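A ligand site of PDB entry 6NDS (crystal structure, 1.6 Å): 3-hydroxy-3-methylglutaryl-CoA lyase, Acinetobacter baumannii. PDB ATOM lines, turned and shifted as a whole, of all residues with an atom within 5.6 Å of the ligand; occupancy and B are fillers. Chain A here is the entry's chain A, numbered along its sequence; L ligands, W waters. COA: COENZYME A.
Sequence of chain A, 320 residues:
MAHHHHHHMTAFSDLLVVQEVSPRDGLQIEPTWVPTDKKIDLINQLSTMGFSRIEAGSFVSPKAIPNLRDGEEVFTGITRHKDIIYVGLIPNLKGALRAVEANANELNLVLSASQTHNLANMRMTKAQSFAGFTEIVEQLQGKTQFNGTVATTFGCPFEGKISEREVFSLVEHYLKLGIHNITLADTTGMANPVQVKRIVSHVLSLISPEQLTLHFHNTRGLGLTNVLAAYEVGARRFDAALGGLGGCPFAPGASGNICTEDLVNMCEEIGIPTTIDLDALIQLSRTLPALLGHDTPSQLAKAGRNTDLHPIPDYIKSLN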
ATOM      1  N   ARG A  24      -5.400 -10.566 -30.130  1.00  0.00           N
ATOM      2  CA  ARG A  24      -5.084 -10.403 -28.713  1.00  0.00           C
ATOM      3  C   ARG A  24      -5.281  -8.945 -28.301  1.00  0.00           C
ATOM      4  O   ARG A  24      -6.250  -8.637 -27.595  1.00  0.00           O
ATOM      5  CB  ARG A  24      -3.654 -10.886 -28.453  1.00  0.00           C
ATOM      6  CG  ARG A  24      -3.268 -11.110 -26.976  1.00  0.00           C
ATOM      7  CD  ARG A  24      -3.021  -9.797 -26.224  1.00  0.00           C
ATOM      8  NE  ARG A  24      -1.880  -9.053 -26.752  1.00  0.00           N
ATOM      9  CZ  ARG A  24      -1.527  -7.837 -26.334  1.00  0.00           C
ATOM     10  NH1 ARG A  24      -2.237  -7.233 -25.392  1.00  0.00           N
ATOM     11  NH2 ARG A  24      -0.464  -7.242 -26.857  1.00  0.00           N
ATOM     12  N   GLN A  28      -8.998  -7.752 -26.764  1.00  0.00           N
ATOM     13  CA  GLN A  28      -9.062  -7.758 -25.313  1.00  0.00           C
ATOM     14  C   GLN A  28      -9.895  -6.603 -24.765  1.00  0.00           C
ATOM     15  O   GLN A  28     -10.522  -6.729 -23.706  1.00  0.00           O
ATOM     16  CB  GLN A  28      -7.651  -7.733 -24.717  1.00  0.00           C
ATOM     17  CG  GLN A  28      -6.909  -6.471 -24.986  1.00  0.00           C
ATOM     18  CD  GLN A  28      -5.470  -6.518 -24.510  1.00  0.00           C
ATOM     19  OE1 GLN A  28      -4.916  -7.585 -24.208  1.00  0.00           O
ATOM     20  NE2 GLN A  28      -4.849  -5.341 -24.443  1.00  0.00           N
ATOM     21  N   SER A  58      -4.239 -14.709 -25.342  1.00  0.00           N
ATOM     22  CA  SER A  58      -3.567 -14.535 -24.065  1.00  0.00           C
ATOM     23  C   SER A  58      -3.943 -15.666 -23.141  1.00  0.00           C
ATOM     24  O   SER A  58      -5.024 -16.255 -23.259  1.00  0.00           O
ATOM     25  CB  SER A  58      -3.955 -13.216 -23.372  1.00  0.00           C
ATOM     26  OG  SER A  58      -3.557 -12.106 -24.117  1.00  0.00           O
ATOM     27  N   PHE A  59      -3.073 -15.929 -22.173  1.00  0.00           N
ATOM     28  CA  PHE A  59      -3.353 -16.899 -21.113  1.00  0.00           C
ATOM     29  C   PHE A  59      -3.299 -16.160 -19.784  1.00  0.00           C
ATOM     30  O   PHE A  59      -2.346 -16.291 -19.022  1.00  0.00           O
ATOM     31  CB  PHE A  59      -2.394 -18.082 -21.215  1.00  0.00           C
ATOM     32  CG  PHE A  59      -2.579 -18.853 -22.492  1.00  0.00           C
ATOM     33  CD1 PHE A  59      -3.516 -19.873 -22.564  1.00  0.00           C
ATOM     34  CD2 PHE A  59      -1.894 -18.494 -23.641  1.00  0.00           C
ATOM     35  CE1 PHE A  59      -3.729 -20.560 -23.750  1.00  0.00           C
ATOM     36  CE2 PHE A  59      -2.109 -19.175 -24.835  1.00  0.00           C
ATOM     37  CZ  PHE A  59      -3.026 -20.211 -24.886  1.00  0.00           C
ATOM     38  N   VAL A  60      -4.338 -15.364 -19.531  1.00  0.00           N
ATOM     39  CA  VAL A  60      -4.404 -14.463 -18.394  1.00  0.00           C
ATOM     40  C   VAL A  60      -5.695 -14.748 -17.629  1.00  0.00           C
ATOM     41  O   VAL A  60      -6.551 -15.520 -18.074  1.00  0.00           O
ATOM     42  CB  VAL A  60      -4.350 -12.975 -18.830  1.00  0.00           C
ATOM     43  CG1 VAL A  60      -3.046 -12.677 -19.553  1.00  0.00           C
ATOM     44  CG2 VAL A  60      -5.553 -12.633 -19.714  1.00  0.00           C
ATOM     45  N   SER A  61      -5.804 -14.131 -16.466  1.00  0.00           N
ATOM     46  CA  SER A  61      -6.980 -14.328 -15.620  1.00  0.00           C
ATOM     47  C   SER A  61      -8.247 -13.994 -16.392  1.00  0.00           C
ATOM     48  O   SER A  61      -8.313 -12.936 -17.021  1.00  0.00           O
ATOM     49  CB  SER A  61      -6.893 -13.440 -14.372  1.00  0.00           C
ATOM     50  OG  SER A  61      -8.127 -13.451 -13.680  1.00  0.00           O
ATOM     51  N   PRO A  62      -9.256 -14.854 -16.369  1.00  0.00           N
ATOM     52  CA  PRO A  62     -10.536 -14.476 -16.994  1.00  0.00           C
ATOM     53  C   PRO A  62     -11.239 -13.360 -16.246  1.00  0.00           C
ATOM     54  O   PRO A  62     -12.112 -12.704 -16.824  1.00  0.00           O
ATOM     55  CB  PRO A  62     -11.347 -15.785 -16.952  1.00  0.00           C
ATOM     56  CG  PRO A  62     -10.801 -16.496 -15.747  1.00  0.00           C
ATOM     57  CD  PRO A  62      -9.332 -16.178 -15.725  1.00  0.00           C
ATOM     58  N   LYS A  63     -10.886 -13.117 -14.970  1.00  0.00           N
ATOM     59  CA  LYS A  63     -11.437 -11.960 -14.273  1.00  0.00           C
ATOM     60  C   LYS A  63     -10.831 -10.666 -14.782  1.00  0.00           C
ATOM     61  O   LYS A  63     -11.503  -9.631 -14.812  1.00  0.00           O
ATOM     62  CB  LYS A  63     -11.214 -12.099 -12.766  1.00  0.00           C
ATOM     63  CG  LYS A  63     -11.963 -13.246 -12.128  1.00  0.00           C
ATOM     64  CD  LYS A  63     -11.695 -13.281 -10.624  1.00  0.00           C
ATOM     65  CE  LYS A  63     -12.451 -14.406  -9.943  1.00  0.00           C
ATOM     66  NZ  LYS A  63     -12.262 -14.374  -8.470  1.00  0.00           N
ATOM     67  N   ALA A  64      -9.564 -10.705 -15.180  1.00  0.00           N
ATOM     68  CA  ALA A  64      -8.886  -9.536 -15.722  1.00  0.00           C
ATOM     69  C   ALA A  64      -9.306  -9.234 -17.148  1.00  0.00           C
ATOM     70  O   ALA A  64      -9.595  -8.086 -17.490  1.00  0.00           O
ATOM     71  CB  ALA A  64      -7.372  -9.753 -15.662  1.00  0.00           C
ATOM     72  N   ILE A  65      -9.334 -10.251 -18.015  1.00  0.00           N
ATOM     73  CA  ILE A  65      -9.591 -10.047 -19.441  1.00  0.00           C
ATOM     74  C   ILE A  65     -10.607 -11.086 -19.892  1.00  0.00           C
ATOM     75  O   ILE A  65     -10.228 -12.087 -20.521  1.00  0.00           O
ATOM     76  CB  ILE A  65      -8.286 -10.132 -20.269  1.00  0.00           C
ATOM     77  CG1 ILE A  65      -7.222  -9.192 -19.701  1.00  0.00           C
ATOM     78  CG2 ILE A  65      -8.539  -9.817 -21.756  1.00  0.00           C
ATOM     79  CD1 ILE A  65      -7.436  -7.716 -20.034  1.00  0.00           C
ATOM     80  N   LEU A  89       0.282 -14.380 -25.268  1.00  0.00           N
ATOM     81  CA  LEU A  89       0.724 -13.452 -24.226  1.00  0.00           C
ATOM     82  C   LEU A  89       0.578 -14.101 -22.852  1.00  0.00           C
ATOM     83  O   LEU A  89      -0.470 -14.676 -22.531  1.00  0.00           O
ATOM     84  CB  LEU A  89      -0.089 -12.153 -24.270  1.00  0.00           C
ATOM     85  CG  LEU A  89       0.282 -11.094 -23.217  1.00  0.00           C
ATOM     86  CD1 LEU A  89       0.068  -9.704 -23.786  1.00  0.00           C
ATOM     87  CD2 LEU A  89      -0.556 -11.232 -21.946  1.00  0.00           C
ATOM     88  N   PRO A  91       1.460 -13.725 -18.487  1.00  0.00           N
ATOM     89  CA  PRO A  91       1.879 -12.841 -17.394  1.00  0.00           C
ATOM     90  C   PRO A  91       2.659 -13.537 -16.281  1.00  0.00           C
ATOM     91  O   PRO A  91       3.310 -12.853 -15.491  1.00  0.00           O
ATOM     92  CB  PRO A  91       0.543 -12.328 -16.858  1.00  0.00           C
ATOM     93  CG  PRO A  91      -0.340 -13.574 -16.966  1.00  0.00           C
ATOM     94  CD  PRO A  91       0.167 -14.362 -18.193  1.00  0.00           C
ATOM     95  N   ASN A  92       2.550 -14.862 -16.179  1.00  0.00           N
ATOM     96  CA  ASN A  92       3.086 -15.598 -15.039  1.00  0.00           C
ATOM     97  C   ASN A  92       3.191 -17.089 -15.386  1.00  0.00           C
ATOM     98  O   ASN A  92       2.874 -17.509 -16.507  1.00  0.00           O
ATOM     99  CB  ASN A  92       2.228 -15.389 -13.783  1.00  0.00           C
ATOM    100  CG  ASN A  92       0.776 -15.874 -13.964  1.00  0.00           C
ATOM    101  OD1 ASN A  92       0.433 -16.523 -14.939  1.00  0.00           O
ATOM    102  ND2 ASN A  92      -0.068 -15.529 -13.004  1.00  0.00           N
ATOM    103  N   LYS A  94       1.531 -19.803 -14.333  1.00  0.00           N
ATOM    104  CA  LYS A  94       0.286 -20.502 -14.646  1.00  0.00           C
ATOM    105  C   LYS A  94      -0.100 -20.301 -16.101  1.00  0.00           C
ATOM    106  O   LYS A  94      -0.504 -21.249 -16.780  1.00  0.00           O
ATOM    107  CB  LYS A  94      -0.835 -20.013 -13.723  1.00  0.00           C
ATOM    108  N   GLY A  95       0.026 -19.071 -16.612  1.00  0.00           N
ATOM    109  CA  GLY A  95      -0.282 -18.809 -18.009  1.00  0.00           C
ATOM    110  C   GLY A  95       0.680 -19.483 -18.956  1.00  0.00           C
ATOM    111  O   GLY A  95       0.277 -19.988 -20.013  1.00  0.00           O
ATOM    112  N   ARG A  98      -0.357 -23.110 -19.275  1.00  0.00           N
ATOM    113  CA  ARG A  98      -1.535 -23.202 -20.131  1.00  0.00           C
ATOM    114  C   ARG A  98      -1.149 -23.061 -21.602  1.00  0.00           C
ATOM    115  O   ARG A  98      -1.638 -23.803 -22.451  1.00  0.00           O
ATOM    116  CB  ARG A  98      -2.551 -22.107 -19.776  1.00  0.00           C
ATOM    117  CG  ARG A  98      -3.286 -22.251 -18.425  1.00  0.00           C
ATOM    118  CD  ARG A  98      -4.108 -20.990 -18.130  1.00  0.00           C
ATOM    119  NE  ARG A  98      -5.092 -20.693 -19.181  1.00  0.00           N
ATOM    120  CZ  ARG A  98      -5.606 -19.494 -19.426  1.00  0.00           C
ATOM    121  NH1 ARG A  98      -5.229 -18.439 -18.715  1.00  0.00           N
ATOM    122  NH2 ARG A  98      -6.490 -19.332 -20.411  1.00  0.00           N
ATOM    123  N   VAL A 110       5.267 -10.487 -20.460  1.00  0.00           N
ATOM    124  CA  VAL A 110       5.007  -9.040 -20.414  1.00  0.00           C
ATOM    125  C   VAL A 110       5.125  -8.516 -18.990  1.00  0.00           C
ATOM    126  O   VAL A 110       4.501  -9.058 -18.074  1.00  0.00           O
ATOM    127  CB  VAL A 110       3.616  -8.697 -20.995  1.00  0.00           C
ATOM    128  CG1 VAL A 110       3.367  -7.180 -20.890  1.00  0.00           C
ATOM    129  CG2 VAL A 110       3.514  -9.150 -22.448  1.00  0.00           C
ATOM    130  N   ASN A 121      -1.951  -3.628 -13.812  1.00  0.00           N
ATOM    131  CA  ASN A 121      -2.199  -4.558 -14.908  1.00  0.00           C
ATOM    132  C   ASN A 121      -1.966  -6.009 -14.500  1.00  0.00           C
ATOM    133  O   ASN A 121      -2.765  -6.891 -14.863  1.00  0.00           O
ATOM    134  CB  ASN A 121      -1.280  -4.208 -16.090  1.00  0.00           C
ATOM    135  CG  ASN A 121      -1.744  -4.806 -17.396  1.00  0.00           C
ATOM    136  OD1 ASN A 121      -2.940  -4.901 -17.675  1.00  0.00           O
ATOM    137  ND2 ASN A 121      -0.786  -5.220 -18.222  1.00  0.00           N
ATOM    138  N   MET A 122      -0.894  -6.271 -13.762  1.00  0.00           N
ATOM    139  CA  MET A 122      -0.477  -7.615 -13.391  1.00  0.00           C
ATOM    140  C   MET A 122      -0.649  -7.901 -11.906  1.00  0.00           C
ATOM    141  O   MET A 122      -0.406  -9.032 -11.488  1.00  0.00           O
ATOM    142  CB  MET A 122       0.997  -7.829 -13.755  1.00  0.00           C
ATOM    143  CG  MET A 122       1.322  -7.654 -15.223  1.00  0.00           C
ATOM    144  SD  MET A 122       0.429  -8.863 -16.214  1.00  0.00           S
ATOM    145  CE  MET A 122       1.168  -8.630 -17.829  1.00  0.00           C
ATOM    146  N   ARG A 123      -1.026  -6.894 -11.111  1.00  0.00           N
ATOM    147  CA  ARG A 123      -1.229  -7.050  -9.676  1.00  0.00           C
ATOM    148  C   ARG A 123       0.022  -7.600  -9.001  1.00  0.00           C
ATOM    149  O   ARG A 123      -0.052  -8.385  -8.042  1.00  0.00           O
ATOM    150  CB  ARG A 123      -2.462  -7.913  -9.393  1.00  0.00           C
ATOM    151  CG  ARG A 123      -3.754  -7.206  -9.821  1.00  0.00           C
ATOM    152  CD  ARG A 123      -4.931  -8.154  -9.890  1.00  0.00           C
ATOM    153  NE  ARG A 123      -5.025  -8.959  -8.677  1.00  0.00           N
ATOM    154  CZ  ARG A 123      -5.738  -8.617  -7.605  1.00  0.00           C
ATOM    155  NH1 ARG A 123      -6.428  -7.485  -7.600  1.00  0.00           N
ATOM    156  NH2 ARG A 123      -5.755  -9.413  -6.544  1.00  0.00           N
ATOM    157  N   MET A 124       1.185  -7.174  -9.482  1.00  0.00           N
ATOM    158  CA  MET A 124       2.432  -7.493  -8.807  1.00  0.00           C
ATOM    159  C   MET A 124       3.501  -6.502  -9.230  1.00  0.00           C
ATOM    160  O   MET A 124       3.371  -5.798 -10.240  1.00  0.00           O
ATOM    161  CB  MET A 124       2.885  -8.929  -9.086  1.00  0.00           C
ATOM    162  CG  MET A 124       2.982  -9.290 -10.541  1.00  0.00           C
ATOM    163  SD  MET A 124       3.362 -11.048 -10.813  1.00  0.00           S
ATOM    164  CE  MET A 124       2.553 -11.287 -12.387  1.00  0.00           C
ATOM    165  N   CYS A 248      -5.304  -1.466 -24.019  1.00  0.00           N
ATOM    166  CA  CYS A 248      -5.318  -2.245 -22.784  1.00  0.00           C
ATOM    167  C   CYS A 248      -6.382  -1.703 -21.839  1.00  0.00           C
ATOM    168  O   CYS A 248      -6.420  -0.483 -21.600  1.00  0.00           O
ATOM    169  CB  CYS A 248      -3.955  -2.219 -22.099  1.00  0.00           C
ATOM    170  SG  CYS A 248      -3.908  -2.982 -20.432  1.00  0.00           S
ATOM    171  N   PRO A 249      -7.243  -2.561 -21.280  1.00  0.00           N
ATOM    172  CA  PRO A 249      -8.317  -2.056 -20.407  1.00  0.00           C
ATOM    173  C   PRO A 249      -7.820  -1.483 -19.091  1.00  0.00           C
ATOM    174  O   PRO A 249      -8.572  -0.744 -18.443  1.00  0.00           O
ATOM    175  CB  PRO A 249      -9.190  -3.303 -20.167  1.00  0.00           C
ATOM    176  CG  PRO A 249      -8.795  -4.271 -21.254  1.00  0.00           C
ATOM    177  CD  PRO A 249      -7.353  -4.007 -21.512  1.00  0.00           C
ATOM    178  N   PHE A 250      -6.585  -1.784 -18.688  1.00  0.00           N
ATOM    179  CA  PHE A 250      -6.048  -1.312 -17.415  1.00  0.00           C
ATOM    180  C   PHE A 250      -5.054  -0.180 -17.581  1.00  0.00           C
ATOM    181  O   PHE A 250      -4.508   0.306 -16.589  1.00  0.00           O
ATOM    182  CB  PHE A 250      -5.422  -2.489 -16.659  1.00  0.00           C
ATOM    183  CG  PHE A 250      -6.389  -3.607 -16.378  1.00  0.00           C
ATOM    184  CD1 PHE A 250      -7.386  -3.448 -15.419  1.00  0.00           C
ATOM    185  CD2 PHE A 250      -6.332  -4.789 -17.096  1.00  0.00           C
ATOM    186  CE1 PHE A 250      -8.288  -4.472 -15.165  1.00  0.00           C
ATOM    187  CE2 PHE A 250      -7.248  -5.814 -16.839  1.00  0.00           C
ATOM    188  CZ  PHE A 250      -8.225  -5.647 -15.880  1.00  0.00           C
HETATM  189  N1A COA L   1      -4.497 -17.555 -16.281  1.00  0.00           N
HETATM  190  C2A COA L   1      -5.634 -17.938 -15.676  1.00  0.00           C
HETATM  191  N3A COA L   1      -5.927 -17.987 -14.380  1.00  0.00           N
HETATM  192  C4A COA L   1      -4.887 -17.561 -13.640  1.00  0.00           C
HETATM  193  C5A COA L   1      -3.660 -17.117 -14.113  1.00  0.00           C
HETATM  194  C6A COA L   1      -3.467 -17.119 -15.506  1.00  0.00           C
HETATM  195  N6A COA L   1      -2.342 -16.731 -16.092  1.00  0.00           N
HETATM  196  N7A COA L   1      -2.839 -16.769 -13.055  1.00  0.00           N
HETATM  197  C8A COA L   1      -3.568 -16.993 -11.975  1.00  0.00           C
HETATM  198  N9A COA L   1      -4.814 -17.466 -12.279  1.00  0.00           N
HETATM  199  C1B COA L   1      -5.877 -17.854 -11.335  1.00  0.00           C
HETATM  200  C2B COA L   1      -5.468 -18.916 -10.327  1.00  0.00           C
HETATM  201  O2B COA L   1      -5.461 -20.232 -10.813  1.00  0.00           O
HETATM  202  C3B COA L   1      -6.502 -18.651  -9.234  1.00  0.00           C
HETATM  203  O3B COA L   1      -7.791 -19.076  -9.655  1.00  0.00           O
HETATM  204  P3B COA L   1      -8.768 -19.264  -8.382  1.00  0.00           P
HETATM  205  O7A COA L   1      -9.360 -17.901  -8.042  1.00  0.00           O
HETATM  206  O8A COA L   1      -7.897 -19.799  -7.268  1.00  0.00           O
HETATM  207  O9A COA L   1      -9.827 -20.256  -8.801  1.00  0.00           O
HETATM  208  C4B COA L   1      -6.391 -17.134  -9.177  1.00  0.00           C
HETATM  209  O4B COA L   1      -6.274 -16.733 -10.579  1.00  0.00           O
HETATM  210  C5B COA L   1      -5.133 -16.703  -8.467  1.00  0.00           C
HETATM  211  O5B COA L   1      -5.093 -15.264  -8.408  1.00  0.00           O
HETATM  212  P1A COA L   1      -3.666 -14.602  -8.147  1.00  0.00           P
HETATM  213  O1A COA L   1      -2.578 -15.562  -8.465  1.00  0.00           O
HETATM  214  O2A COA L   1      -3.675 -13.900  -6.826  1.00  0.00           O
HETATM  215  O3A COA L   1      -3.705 -13.516  -9.326  1.00  0.00           O
HETATM  216  P2A COA L   1      -4.541 -12.167  -9.504  1.00  0.00           P
HETATM  217  O4A COA L   1      -3.955 -11.118  -8.617  1.00  0.00           O
HETATM  218  O5A COA L   1      -6.000 -12.450  -9.417  1.00  0.00           O
HETATM  219  O6A COA L   1      -4.195 -11.850 -11.041  1.00  0.00           O
HETATM  220  CBP COA L   1      -2.787 -11.931 -12.970  1.00  0.00           C
HETATM  221  CCP COA L   1      -2.816 -11.743 -11.454  1.00  0.00           C
HETATM  222  CDP COA L   1      -1.388 -11.653 -13.520  1.00  0.00           C
HETATM  223  CEP COA L   1      -3.170 -13.377 -13.304  1.00  0.00           C
HETATM  224  CAP COA L   1      -3.807 -10.961 -13.564  1.00  0.00           C
HETATM  225  OAP COA L   1      -3.551  -9.656 -13.070  1.00  0.00           O
HETATM  226  C9P COA L   1      -3.777 -10.916 -15.092  1.00  0.00           C
HETATM  227  O9P COA L   1      -4.199 -11.855 -15.747  1.00  0.00           O
HETATM  228  N8P COA L   1      -3.279  -9.814 -15.632  1.00  0.00           N
HETATM  229  C7P COA L   1      -3.077  -9.658 -17.067  1.00  0.00           C
HETATM  230  C6P COA L   1      -4.027  -8.657 -17.657  1.00  0.00           C
HETATM  231  C5P COA L   1      -3.713  -8.367 -19.116  1.00  0.00           C
HETATM  232  O5P COA L   1      -3.557  -9.288 -19.916  1.00  0.00           O
HETATM  233  N4P COA L   1      -3.627  -7.084 -19.467  1.00  0.00           N
HETATM  234  C3P COA L   1      -3.511  -6.619 -20.836  1.00  0.00           C
HETATM  235  C2P COA L   1      -2.281  -7.166 -21.530  1.00  0.00           C
HETATM  236  S1P COA L   1      -0.778  -6.836 -20.583  1.00  0.00           S
HETATM  237  O   HOH W   1      -8.424 -19.043 -13.588  1.00  0.00           O
HETATM  238  O   HOH W   2      -4.340  -9.956 -22.598  1.00  0.00           O
HETATM  239  O   HOH W   3      -1.523 -14.041  -5.198  1.00  0.00           O
HETATM  240  O   HOH W   4      -6.087  -7.810 -13.024  1.00  0.00           O
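An oxygen (O4A) of the ligand lies within salt-bridge range of the guanidinium group (NE) of Arg 123 (2.4 Å). The guanidinium group of Arg 98 sits at hydrogen-bond distance from a nitrogen (N1A) of the ligand. The backbone carbonyl oxygen (O) of Asn 121 sits at hydrogen-bond distance from a nitrogen (N8P) of the ligand (3.1 Å). S1P of the ligand lies close to ND2 of Asn 121 (2.9 Å). O9P of the ligand lies within hydrogen-bond range of N of Ser 61 (2.9 Å). N6A of the ligand sits at hydrogen-bond distance from O of Phe 59, 3.0 Å away. OD1 of Asn 92 is in hydrogen-bond range of N6A of the ligand (3.0 Å).
The guanidinium group (NH1) of Arg 98 is in hydrogen-bond range of the backbone carbonyl oxygen (O) of Val 60 (3.3 Å). The side-chain amide oxygen (OD1) of Asn 121 is in hydrogen-bond range of the side-chain sulfur (SG) of Cys 248 (3.5 Å). The backbone NH (N) of Ala 64 lies within hydrogen-bond range of the side-chain hydroxyl (OG) of Ser 61 (3.4 Å). The backbone NH (N) of Lys 63 lies within hydrogen-bond range of the side-chain hydroxyl (OG) of Ser 61 (3.1 Å). The backbone NH (N) of Phe 59 lies within hydrogen-bond range of the backbone carbonyl oxygen (O) of Leu 89 (2.9 Å). The side-chain amide oxygen (OD1) of Asn 92 lies within hydrogen-bond range of the backbone NH (N) of Gly 95, at 3.1 Å. The side-chain sulfur of Cys 248 lies close to the backbone NH of Phe 250 (3.4 Å). The side-chain amide oxygen (OE1) of Gln 28 sits at hydrogen-bond distance from the guanidinium group (NH1) of Arg 24 (3.0 Å).
O of Val 60 lies close to N1A of the ligand, at 3.4 Å. A nitrogen (N6A) of the ligand lies close to the backbone NH of Gly 95, at 3.4 Å. Arg 24 touches the ligand. Gln 28 touches the ligand (OE1 to C3P, 3.8 Å). CB of Ala 64 touches O9P of the ligand, at 3.8 Å. CG1 of Ile 65 touches C5P of the ligand (3.7 Å). Pro 91 touches the ligand. Lys 94 touches the ligand (CB to N7A, 3.9 Å). Met 122 touches the ligand. Cys 248 touches the ligand. Hydrophobic or aromatic side chains that line the ligand: Val 60, Ala 64, Ile 65, Pro 91 and Met 122. 16 residues have an atom within 4 Å of the ligand: Arg 24, Gln 28, Phe 59, Val 60, Ser 61, Ala 64, Ile 65, Pro 91, Asn 92, Lys 94, Gly 95, Arg 98, Asn 121, Met 122, Arg 123 and Cys 248. Along chain A the residues within 4 Å of the ligand span positions 24 to 248. The nearest printed residue that does not touch the ligand is Pro 62 (4.1 Å).
Water W2 lies within hydrogen-bond range of the side-chain hydroxyl of Ser 58 (2.7 Å), an oxygen (O5P) of the ligand (2.9 Å) and the side-chain amide oxygen of Gln 28 (2.9 Å).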
